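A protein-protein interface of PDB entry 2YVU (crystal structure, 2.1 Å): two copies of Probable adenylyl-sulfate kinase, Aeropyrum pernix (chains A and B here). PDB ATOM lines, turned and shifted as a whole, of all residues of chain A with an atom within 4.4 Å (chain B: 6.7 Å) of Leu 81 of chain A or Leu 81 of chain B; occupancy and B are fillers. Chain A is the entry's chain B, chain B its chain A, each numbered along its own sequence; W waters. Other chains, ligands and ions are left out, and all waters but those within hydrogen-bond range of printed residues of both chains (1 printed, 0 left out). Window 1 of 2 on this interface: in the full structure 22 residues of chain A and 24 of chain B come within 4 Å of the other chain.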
ATOM      1  N   GLU A  45      -2.682  30.515   7.016  1.00  0.00           N
ATOM      2  CA  GLU A  45      -3.205  30.742   5.680  1.00  0.00           C
ATOM      3  C   GLU A  45      -2.869  32.175   5.322  1.00  0.00           C
ATOM      4  O   GLU A  45      -3.059  33.097   6.135  1.00  0.00           O
ATOM      5  CB  GLU A  45      -4.732  30.562   5.612  1.00  0.00           C
ATOM      6  CG  GLU A  45      -5.247  29.139   5.692  1.00  0.00           C
ATOM      7  CD  GLU A  45      -4.833  28.270   4.486  1.00  0.00           C
ATOM      8  OE1 GLU A  45      -4.368  28.816   3.470  1.00  0.00           O
ATOM      9  OE2 GLU A  45      -5.000  27.037   4.555  1.00  0.00           O
ATOM     10  N   ILE A  77     -14.046  35.527   5.655  1.00  0.00           N
ATOM     11  CA  ILE A  77     -13.271  34.302   5.466  1.00  0.00           C
ATOM     12  C   ILE A  77     -12.163  34.215   6.524  1.00  0.00           C
ATOM     13  O   ILE A  77     -11.926  33.151   7.082  1.00  0.00           O
ATOM     14  CB  ILE A  77     -12.635  34.243   4.058  1.00  0.00           C
ATOM     15  CG1 ILE A  77     -13.738  34.115   3.003  1.00  0.00           C
ATOM     16  CG2 ILE A  77     -11.720  33.043   3.948  1.00  0.00           C
ATOM     17  CD1 ILE A  77     -13.274  34.330   1.545  1.00  0.00           C
ATOM     18  N   ALA A  78     -11.486  35.332   6.793  1.00  0.00           N
ATOM     19  CA  ALA A  78     -10.443  35.355   7.822  1.00  0.00           C
ATOM     20  C   ALA A  78     -11.076  35.062   9.192  1.00  0.00           C
ATOM     21  O   ALA A  78     -10.506  34.334  10.004  1.00  0.00           O
ATOM     22  CB  ALA A  78      -9.741  36.724   7.847  1.00  0.00           C
ATOM     23  N   ARG A  79     -12.258  35.622   9.440  1.00  0.00           N
ATOM     24  CA  ARG A  79     -12.968  35.381  10.706  1.00  0.00           C
ATOM     25  C   ARG A  79     -13.281  33.876  10.897  1.00  0.00           C
ATOM     26  O   ARG A  79     -13.061  33.339  11.967  1.00  0.00           O
ATOM     27  CB  ARG A  79     -14.265  36.214  10.736  1.00  0.00           C
ATOM     28  CG  ARG A  79     -15.196  35.969  11.935  1.00  0.00           C
ATOM     29  CD  ARG A  79     -16.236  37.110  12.061  1.00  0.00           C
ATOM     30  NE  ARG A  79     -17.297  36.813  13.032  1.00  0.00           N
ATOM     31  CZ  ARG A  79     -18.241  37.675  13.412  1.00  0.00           C
ATOM     32  NH1 ARG A  79     -18.272  38.915  12.921  1.00  0.00           N
ATOM     33  NH2 ARG A  79     -19.184  37.288  14.267  1.00  0.00           N
ATOM     34  N   LEU A  80     -13.803  33.200   9.867  1.00  0.00           N
ATOM     35  CA  LEU A  80     -14.091  31.765   9.990  1.00  0.00           C
ATOM     36  C   LEU A  80     -12.802  30.966  10.246  1.00  0.00           C
ATOM     37  O   LEU A  80     -12.746  30.127  11.129  1.00  0.00           O
ATOM     38  CB  LEU A  80     -14.779  31.214   8.730  1.00  0.00           C
ATOM     39  CG  LEU A  80     -16.172  31.735   8.391  1.00  0.00           C
ATOM     40  CD1 LEU A  80     -16.776  30.941   7.218  1.00  0.00           C
ATOM     41  CD2 LEU A  80     -17.043  31.601   9.585  1.00  0.00           C
ATOM     42  N   LEU A  81     -11.761  31.223   9.474  1.00  0.00           N
ATOM     43  CA  LEU A  81     -10.516  30.497   9.702  1.00  0.00           C
ATOM     44  C   LEU A  81      -9.929  30.749  11.100  1.00  0.00           C
ATOM     45  O   LEU A  81      -9.625  29.803  11.838  1.00  0.00           O
ATOM     46  CB  LEU A  81      -9.503  30.876   8.627  1.00  0.00           C
ATOM     47  CG  LEU A  81      -9.865  30.431   7.196  1.00  0.00           C
ATOM     48  CD1 LEU A  81      -8.963  31.156   6.217  1.00  0.00           C
ATOM     49  CD2 LEU A  81      -9.715  28.902   7.033  1.00  0.00           C
ATOM     50  N   ALA A  82      -9.779  32.013  11.486  1.00  0.00           N
ATOM     51  CA  ALA A  82      -9.198  32.296  12.793  1.00  0.00           C
ATOM     52  C   ALA A  82     -10.030  31.722  13.964  1.00  0.00           C
ATOM     53  O   ALA A  82      -9.469  31.247  14.962  1.00  0.00           O
ATOM     54  CB  ALA A  82      -8.976  33.837  12.974  1.00  0.00           C
ATOM     55  N   ARG A  83     -11.357  31.734  13.850  1.00  0.00           N
ATOM     56  CA  ARG A  83     -12.152  31.209  14.945  1.00  0.00           C
ATOM     57  C   ARG A  83     -12.008  29.704  15.019  1.00  0.00           C
ATOM     58  O   ARG A  83     -12.449  29.079  15.979  1.00  0.00           O
ATOM     59  CB  ARG A  83     -13.629  31.642  14.839  1.00  0.00           C
ATOM     60  CG  ARG A  83     -14.533  30.883  13.867  1.00  0.00           C
ATOM     61  CD  ARG A  83     -15.857  31.642  13.792  1.00  0.00           C
ATOM     62  NE  ARG A  83     -16.940  30.971  13.063  1.00  0.00           N
ATOM     63  CZ  ARG A  83     -18.085  31.578  12.745  1.00  0.00           C
ATOM     64  NH1 ARG A  83     -18.289  32.847  13.104  1.00  0.00           N
ATOM     65  NH2 ARG A  83     -19.006  30.954  12.020  1.00  0.00           N
ATOM     66  N   ASN A  84     -11.382  29.117  14.007  1.00  0.00           N
ATOM     67  CA  ASN A  84     -11.152  27.691  14.039  1.00  0.00           C
ATOM     68  C   ASN A  84      -9.683  27.365  14.261  1.00  0.00           C
ATOM     69  O   ASN A  84      -9.192  26.299  13.877  1.00  0.00           O
ATOM     70  CB  ASN A  84     -11.692  27.029  12.769  1.00  0.00           C
ATOM     71  CG  ASN A  84     -13.184  26.832  12.837  1.00  0.00           C
ATOM     72  OD1 ASN A  84     -13.661  25.937  13.535  1.00  0.00           O
ATOM     73  ND2 ASN A  84     -13.938  27.689  12.146  1.00  0.00           N
ATOM     74  N   GLY A  85      -8.977  28.310  14.872  1.00  0.00           N
ATOM     75  CA  GLY A  85      -7.591  28.091  15.226  1.00  0.00           C
ATOM     76  C   GLY A  85      -6.496  28.486  14.268  1.00  0.00           C
ATOM     77  O   GLY A  85      -5.336  28.264  14.559  1.00  0.00           O
ATOM     78  N   VAL A  86      -6.845  29.084  13.143  1.00  0.00           N
ATOM     79  CA  VAL A  86      -5.841  29.457  12.143  1.00  0.00           C
ATOM     80  C   VAL A  86      -5.300  30.890  12.276  1.00  0.00           C
ATOM     81  O   VAL A  86      -6.018  31.798  12.675  1.00  0.00           O
ATOM     82  CB  VAL A  86      -6.438  29.315  10.724  1.00  0.00           C
ATOM     83  CG1 VAL A  86      -5.398  29.645   9.680  1.00  0.00           C
ATOM     84  CG2 VAL A  86      -6.972  27.909  10.525  1.00  0.00           C
ATOM     85  N   VAL A  88      -4.368  33.786  10.289  1.00  0.00           N
ATOM     86  CA  VAL A  88      -4.648  34.239   8.940  1.00  0.00           C
ATOM     87  C   VAL A  88      -3.871  35.516   8.618  1.00  0.00           C
ATOM     88  O   VAL A  88      -4.023  36.543   9.282  1.00  0.00           O
ATOM     89  CB  VAL A  88      -6.168  34.508   8.747  1.00  0.00           C
ATOM     90  CG1 VAL A  88      -6.452  34.792   7.284  1.00  0.00           C
ATOM     91  CG2 VAL A  88      -7.011  33.298   9.238  1.00  0.00           C
ATOM     92  N   LYS B  12      -7.142  16.813   8.951  1.00  0.00           N
ATOM     93  CA  LYS B  12      -7.976  17.305   7.857  1.00  0.00           C
ATOM     94  C   LYS B  12      -9.455  17.061   8.104  1.00  0.00           C
ATOM     95  O   LYS B  12      -9.850  16.011   8.623  1.00  0.00           O
ATOM     96  CB  LYS B  12      -7.559  16.657   6.536  1.00  0.00           C
ATOM     97  CG  LYS B  12      -6.105  16.903   6.144  1.00  0.00           C
ATOM     98  CD  LYS B  12      -5.812  18.373   5.863  1.00  0.00           C
ATOM     99  CE  LYS B  12      -4.306  18.611   5.664  1.00  0.00           C
ATOM    100  NZ  LYS B  12      -3.935  20.060   5.522  1.00  0.00           N
ATOM    101  N   GLY B  13     -10.278  18.039   7.735  1.00  0.00           N
ATOM    102  CA  GLY B  13     -11.703  17.896   7.939  1.00  0.00           C
ATOM    103  C   GLY B  13     -12.335  17.318   6.691  1.00  0.00           C
ATOM    104  O   GLY B  13     -11.660  16.661   5.899  1.00  0.00           O
ATOM    105  N   GLU B  45     -18.273  24.113  10.907  1.00  0.00           N
ATOM    106  CA  GLU B  45     -18.828  25.342  10.362  1.00  0.00           C
ATOM    107  C   GLU B  45     -19.934  24.952   9.422  1.00  0.00           C
ATOM    108  O   GLU B  45     -19.758  24.070   8.584  1.00  0.00           O
ATOM    109  CB  GLU B  45     -17.802  26.155   9.602  1.00  0.00           C
ATOM    110  CG  GLU B  45     -16.745  26.758  10.492  1.00  0.00           C
ATOM    111  CD  GLU B  45     -17.300  27.872  11.352  1.00  0.00           C
ATOM    112  OE1 GLU B  45     -18.433  28.315  11.096  1.00  0.00           O
ATOM    113  OE2 GLU B  45     -16.598  28.316  12.262  1.00  0.00           O
ATOM    114  N   LEU B  47     -22.212  26.335   6.504  1.00  0.00           N
ATOM    115  CA  LEU B  47     -22.296  27.412   5.540  1.00  0.00           C
ATOM    116  C   LEU B  47     -23.601  27.211   4.788  1.00  0.00           C
ATOM    117  O   LEU B  47     -23.870  26.123   4.286  1.00  0.00           O
ATOM    118  CB  LEU B  47     -21.103  27.381   4.558  1.00  0.00           C
ATOM    119  CG  LEU B  47     -19.686  27.368   5.159  1.00  0.00           C
ATOM    120  CD1 LEU B  47     -18.653  27.230   4.055  1.00  0.00           C
ATOM    121  CD2 LEU B  47     -19.427  28.643   5.953  1.00  0.00           C
ATOM    122  N   TRP B  76     -14.240  27.137  -2.314  1.00  0.00           N
ATOM    123  CA  TRP B  76     -12.914  27.495  -1.852  1.00  0.00           C
ATOM    124  C   TRP B  76     -12.848  27.741  -0.362  1.00  0.00           C
ATOM    125  O   TRP B  76     -11.887  27.324   0.291  1.00  0.00           O
ATOM    126  CB  TRP B  76     -12.415  28.695  -2.618  1.00  0.00           C
ATOM    127  CG  TRP B  76     -11.692  28.239  -3.841  1.00  0.00           C
ATOM    128  CD1 TRP B  76     -12.176  28.166  -5.116  1.00  0.00           C
ATOM    129  CD2 TRP B  76     -10.355  27.738  -3.886  1.00  0.00           C
ATOM    130  NE1 TRP B  76     -11.218  27.655  -5.952  1.00  0.00           N
ATOM    131  CE2 TRP B  76     -10.088  27.385  -5.223  1.00  0.00           C
ATOM    132  CE3 TRP B  76      -9.356  27.555  -2.918  1.00  0.00           C
ATOM    133  CZ2 TRP B  76      -8.853  26.858  -5.625  1.00  0.00           C
ATOM    134  CZ3 TRP B  76      -8.124  27.031  -3.317  1.00  0.00           C
ATOM    135  CH2 TRP B  76      -7.887  26.691  -4.662  1.00  0.00           C
ATOM    136  N   ILE B  77     -13.878  28.402   0.171  1.00  0.00           N
ATOM    137  CA  ILE B  77     -13.959  28.699   1.595  1.00  0.00           C
ATOM    138  C   ILE B  77     -14.034  27.363   2.329  1.00  0.00           C
ATOM    139  O   ILE B  77     -13.392  27.166   3.354  1.00  0.00           O
ATOM    140  CB  ILE B  77     -15.212  29.528   1.916  1.00  0.00           C
ATOM    141  CG1 ILE B  77     -15.120  30.893   1.216  1.00  0.00           C
ATOM    142  CG2 ILE B  77     -15.398  29.646   3.420  1.00  0.00           C
ATOM    143  CD1 ILE B  77     -16.398  31.779   1.326  1.00  0.00           C
ATOM    144  N   ALA B  78     -14.819  26.446   1.788  1.00  0.00           N
ATOM    145  CA  ALA B  78     -14.953  25.116   2.387  1.00  0.00           C
ATOM    146  C   ALA B  78     -13.618  24.367   2.342  1.00  0.00           C
ATOM    147  O   ALA B  78     -13.246  23.694   3.278  1.00  0.00           O
ATOM    148  CB  ALA B  78     -16.014  24.310   1.638  1.00  0.00           C
ATOM    149  N   ARG B  79     -12.904  24.487   1.233  1.00  0.00           N
ATOM    150  CA  ARG B  79     -11.628  23.807   1.083  1.00  0.00           C
ATOM    151  C   ARG B  79     -10.597  24.351   2.092  1.00  0.00           C
ATOM    152  O   ARG B  79      -9.875  23.587   2.748  1.00  0.00           O
ATOM    153  CB  ARG B  79     -11.158  23.969  -0.369  1.00  0.00           C
ATOM    154  CG  ARG B  79      -9.700  23.628  -0.640  1.00  0.00           C
ATOM    155  CD  ARG B  79      -9.432  23.642  -2.152  1.00  0.00           C
ATOM    156  NE  ARG B  79      -8.014  23.531  -2.499  1.00  0.00           N
ATOM    157  CZ  ARG B  79      -7.554  23.390  -3.745  1.00  0.00           C
ATOM    158  NH1 ARG B  79      -8.392  23.332  -4.774  1.00  0.00           N
ATOM    159  NH2 ARG B  79      -6.252  23.321  -3.969  1.00  0.00           N
ATOM    160  N   LEU B  80     -10.541  25.675   2.228  1.00  0.00           N
ATOM    161  CA  LEU B  80      -9.620  26.289   3.167  1.00  0.00           C
ATOM    162  C   LEU B  80      -9.931  25.855   4.597  1.00  0.00           C
ATOM    163  O   LEU B  80      -9.034  25.533   5.360  1.00  0.00           O
ATOM    164  CB  LEU B  80      -9.706  27.809   3.081  1.00  0.00           C
ATOM    165  CG  LEU B  80      -8.625  28.567   2.307  1.00  0.00           C
ATOM    166  CD1 LEU B  80      -8.231  27.833   1.064  1.00  0.00           C
ATOM    167  CD2 LEU B  80      -9.170  29.964   1.976  1.00  0.00           C
ATOM    168  N   LEU B  81     -11.196  25.862   4.973  1.00  0.00           N
ATOM    169  CA  LEU B  81     -11.530  25.470   6.339  1.00  0.00           C
ATOM    170  C   LEU B  81     -11.192  23.995   6.562  1.00  0.00           C
ATOM    171  O   LEU B  81     -10.573  23.616   7.568  1.00  0.00           O
ATOM    172  CB  LEU B  81     -13.022  25.713   6.614  1.00  0.00           C
ATOM    173  CG  LEU B  81     -13.480  27.175   6.816  1.00  0.00           C
ATOM    174  CD1 LEU B  81     -15.005  27.282   6.681  1.00  0.00           C
ATOM    175  CD2 LEU B  81     -13.044  27.671   8.189  1.00  0.00           C
ATOM    176  N   ALA B  82     -11.580  23.164   5.606  1.00  0.00           N
ATOM    177  CA  ALA B  82     -11.364  21.733   5.738  1.00  0.00           C
ATOM    178  C   ALA B  82      -9.896  21.330   5.782  1.00  0.00           C
ATOM    179  O   ALA B  82      -9.533  20.412   6.519  1.00  0.00           O
ATOM    180  CB  ALA B  82     -12.101  20.987   4.617  1.00  0.00           C
ATOM    181  N   ARG B  83      -9.047  21.993   5.004  1.00  0.00           N
ATOM    182  CA  ARG B  83      -7.636  21.642   5.050  1.00  0.00           C
ATOM    183  C   ARG B  83      -7.040  22.079   6.380  1.00  0.00           C
ATOM    184  O   ARG B  83      -5.890  21.751   6.682  1.00  0.00           O
ATOM    185  CB  ARG B  83      -6.848  22.249   3.871  1.00  0.00           C
ATOM    186  CG  ARG B  83      -6.562  23.745   3.902  1.00  0.00           C
ATOM    187  CD  ARG B  83      -6.039  24.126   2.526  1.00  0.00           C
ATOM    188  NE  ARG B  83      -5.513  25.488   2.412  1.00  0.00           N
ATOM    189  CZ  ARG B  83      -5.220  26.049   1.242  1.00  0.00           C
ATOM    190  NH1 ARG B  83      -5.419  25.356   0.121  1.00  0.00           N
ATOM    191  NH2 ARG B  83      -4.712  27.275   1.179  1.00  0.00           N
ATOM    192  N   ASN B  84      -7.810  22.819   7.181  1.00  0.00           N
ATOM    193  CA  ASN B  84      -7.306  23.222   8.489  1.00  0.00           C
ATOM    194  C   ASN B  84      -8.018  22.502   9.616  1.00  0.00           C
ATOM    195  O   ASN B  84      -8.130  23.028  10.714  1.00  0.00           O
ATOM    196  CB  ASN B  84      -7.393  24.740   8.676  1.00  0.00           C
ATOM    197  CG  ASN B  84      -6.322  25.477   7.881  1.00  0.00           C
ATOM    198  OD1 ASN B  84      -5.156  25.492   8.263  1.00  0.00           O
ATOM    199  ND2 ASN B  84      -6.709  26.060   6.760  1.00  0.00           N
ATOM    200  N   GLY B  85      -8.520  21.305   9.323  1.00  0.00           N
ATOM    201  CA  GLY B  85      -9.168  20.488  10.340  1.00  0.00           C
ATOM    202  C   GLY B  85     -10.641  20.671  10.638  1.00  0.00           C
ATOM    203  O   GLY B  85     -11.160  20.035  11.537  1.00  0.00           O
ATOM    204  N   VAL B  86     -11.330  21.498   9.862  1.00  0.00           N
ATOM    205  CA  VAL B  86     -12.728  21.760  10.100  1.00  0.00           C
ATOM    206  C   VAL B  86     -13.695  20.885   9.308  1.00  0.00           C
ATOM    207  O   VAL B  86     -13.477  20.604   8.135  1.00  0.00           O
ATOM    208  CB  VAL B  86     -13.046  23.225   9.754  1.00  0.00           C
ATOM    209  CG1 VAL B  86     -14.506  23.527  10.052  1.00  0.00           C
ATOM    210  CG2 VAL B  86     -12.102  24.158  10.517  1.00  0.00           C
ATOM    211  N   ILE B  87     -14.773  20.474   9.960  1.00  0.00           N
ATOM    212  CA  ILE B  87     -15.822  19.704   9.309  1.00  0.00           C
ATOM    213  C   ILE B  87     -16.760  20.775   8.760  1.00  0.00           C
ATOM    214  O   ILE B  87     -17.391  21.506   9.529  1.00  0.00           O
ATOM    215  CB  ILE B  87     -16.575  18.807  10.322  1.00  0.00           C
ATOM    216  CG1 ILE B  87     -15.635  17.693  10.831  1.00  0.00           C
ATOM    217  CG2 ILE B  87     -17.827  18.205   9.651  1.00  0.00           C
ATOM    218  CD1 ILE B  87     -16.249  16.794  11.920  1.00  0.00           C
ATOM    219  N   VAL B  88     -16.841  20.883   7.437  1.00  0.00           N
ATOM    220  CA  VAL B  88     -17.671  21.918   6.831  1.00  0.00           C
ATOM    221  C   VAL B  88     -18.967  21.360   6.313  1.00  0.00           C
ATOM    222  O   VAL B  88     -18.966  20.550   5.390  1.00  0.00           O
ATOM    223  CB  VAL B  88     -16.953  22.575   5.669  1.00  0.00           C
ATOM    224  CG1 VAL B  88     -17.722  23.867   5.221  1.00  0.00           C
ATOM    225  CG2 VAL B  88     -15.520  22.881   6.083  1.00  0.00           C
ATOM    226  N   ILE B 112      -9.458  16.549  -0.021  1.00  0.00           N
ATOM    227  CA  ILE B 112     -10.493  16.546   1.007  1.00  0.00           C
ATOM    228  C   ILE B 112     -11.724  15.749   0.600  1.00  0.00           C
ATOM    229  O   ILE B 112     -12.246  15.919  -0.499  1.00  0.00           O
ATOM    230  CB  ILE B 112     -10.932  17.995   1.327  1.00  0.00           C
ATOM    231  CG1 ILE B 112      -9.724  18.782   1.817  1.00  0.00           C
ATOM    232  CG2 ILE B 112     -12.043  18.003   2.379  1.00  0.00           C
ATOM    233  CD1 ILE B 112      -9.993  20.257   1.984  1.00  0.00           C
HETATM  234  O   HOH W   1      -4.236  30.398   1.206  1.00  0.00           O
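The backbone NH of Glu 45 of chain B lies within hydrogen-bond range of the backbone carbonyl oxygen of Ile 87 of chain B.
The backbone carbonyl oxygen of Leu 80 of chain B lies within hydrogen-bond range of the side-chain amide nitrogen of Asn 84 of chain B (2.8 Å).
The backbone carbonyl oxygen (O) of Leu 80 of chain A sits at hydrogen-bond distance from the side-chain amide nitrogen (ND2) of Asn 84 of chain A, 2.9 Å away.
NZ of Lys 12 of chain B sits at hydrogen-bond distance from O of Arg 83 of chain B (2.8 Å).
N of Val 86 of chain A sits at hydrogen-bond distance from O of Leu 81 of chain A, at 3.2 Å.
O of Leu 81 of chain B lies within hydrogen-bond range of N of Val 86 of chain B, at 3.2 Å.
Water W1 bridges the side-chain carboxylate (OE1) of Glu 45 of chain A (2.8 Å) and the guanidinium group (NH2) of Arg 83 of chain B (3.2 Å).
Printed residues of chain B that touch a printed residue of chain A: Glu 45, Leu 47, Ile 77, Leu 80, Leu 81, Arg 83, Asn 84 and Val 86.
Hydrophobic or aromatic side chains of chain B that line the printed part of chain A: Leu 47, Ile 77, Leu 81 and Val 86.
Printed residues of chain A that touch a printed residue of chain B: Glu 45, Ile 77, Leu 80, Leu 81, Arg 83, Asn 84 and Val 86.
Hydrophobic or aromatic side chains of chain A within 4 Å of the printed part of chain B: Ile 77, Leu 80, Leu 81 and Val 86.
CD1 of Ile 77 of chain A touches CG1 of Ile 77 of chain B, at 3.9 Å.
Glu 45 of chain B touches Leu 80 of chain A.
Leu 47 of chain B touches Leu 80 of chain A (CD2 to CD1, 3.7 Å).
CD2 of Leu 81 of chain B touches O of Leu 80 of chain A, 3.8 Å away.
CD2 of Leu 81 of chain A touches O of Leu 80 of chain B, 3.8 Å away.
Leu 81 of chain B touches Leu 81 of chain A (CD2 to CD2, 3.7 Å).
Asn 84 of chain A touches Val 86 of chain B.
Asn 84 of chain B touches Val 86 of chain A.
The guanidinium group of Arg 83 of chain A lies within salt-bridge range of the side-chain carboxylate of Glu 45 of chain B (2.8 Å).
The guanidinium group of Arg 83 of chain B lies within salt-bridge range of the side-chain carboxylate of Glu 45 of chain A (2.7 Å).
The side-chain amide nitrogen (ND2) of Asn 84 of chain B sits at hydrogen-bond distance from the side-chain carboxylate (OE2) of Glu 45 of chain A.
OE2 of Glu 45 of chain B sits at hydrogen-bond distance from ND2 of Asn 84 of chain A, at 2.7 Å.
Leu 81 of chain A touches two residues of chain B.
Of the printed residues of chain B, Asn 84 of chain A touches Glu 45 (2.7 Å) and Val 86 (3.7 Å).
Gly 13 of chain B touches none of the printed residues of chain A.
Printed residues of chain A within 4 Å of Glu 45 of chain B: Leu 80 (3.9 Å), Arg 83 (2.8 Å) and Asn 84 (2.7 Å).
Printed residues of chain A within 4 Å of Leu 47 of chain B: Leu 80 (3.7 Å).
Of chain A, only Leu 80 and Leu 81 come within 4 Å of Leu 81 of chain B.
Ala 82 of chain B touches none of the printed residues of chain A.
Of the printed residues of chain A, Arg 83 of chain B touches Glu 45.
The nearest residue of chain A that does not touch Leu 81 of chain B is Asn 84 of chain A (4.1 Å).
The nearest printed residue of chain A that does not touch Glu 45 of chain B is Arg 79 of chain A (6.2 Å).
Ile 77 of chain B touches its own counterpart, Ile 77 of chain A.
Leu 80 of chain A touches Glu 45 of chain B, but with the chains exchanged Glu 45 of chain A does not touch Leu 80 of chain B (4.4 Å).
Leu 80 of chain A touches Leu 81 of chain B, and with the chains exchanged Leu 81 of chain A touches Leu 80 of chain B.
Asn 84 of chain A touches Val 86 of chain B, and with the chains exchanged Val 86 of chain A touches Asn 84 of chain B.
Positions printed for both chains: 45, 77, 78, 79, 80, 81, 82, 83, 84, 85, 86 and 88.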
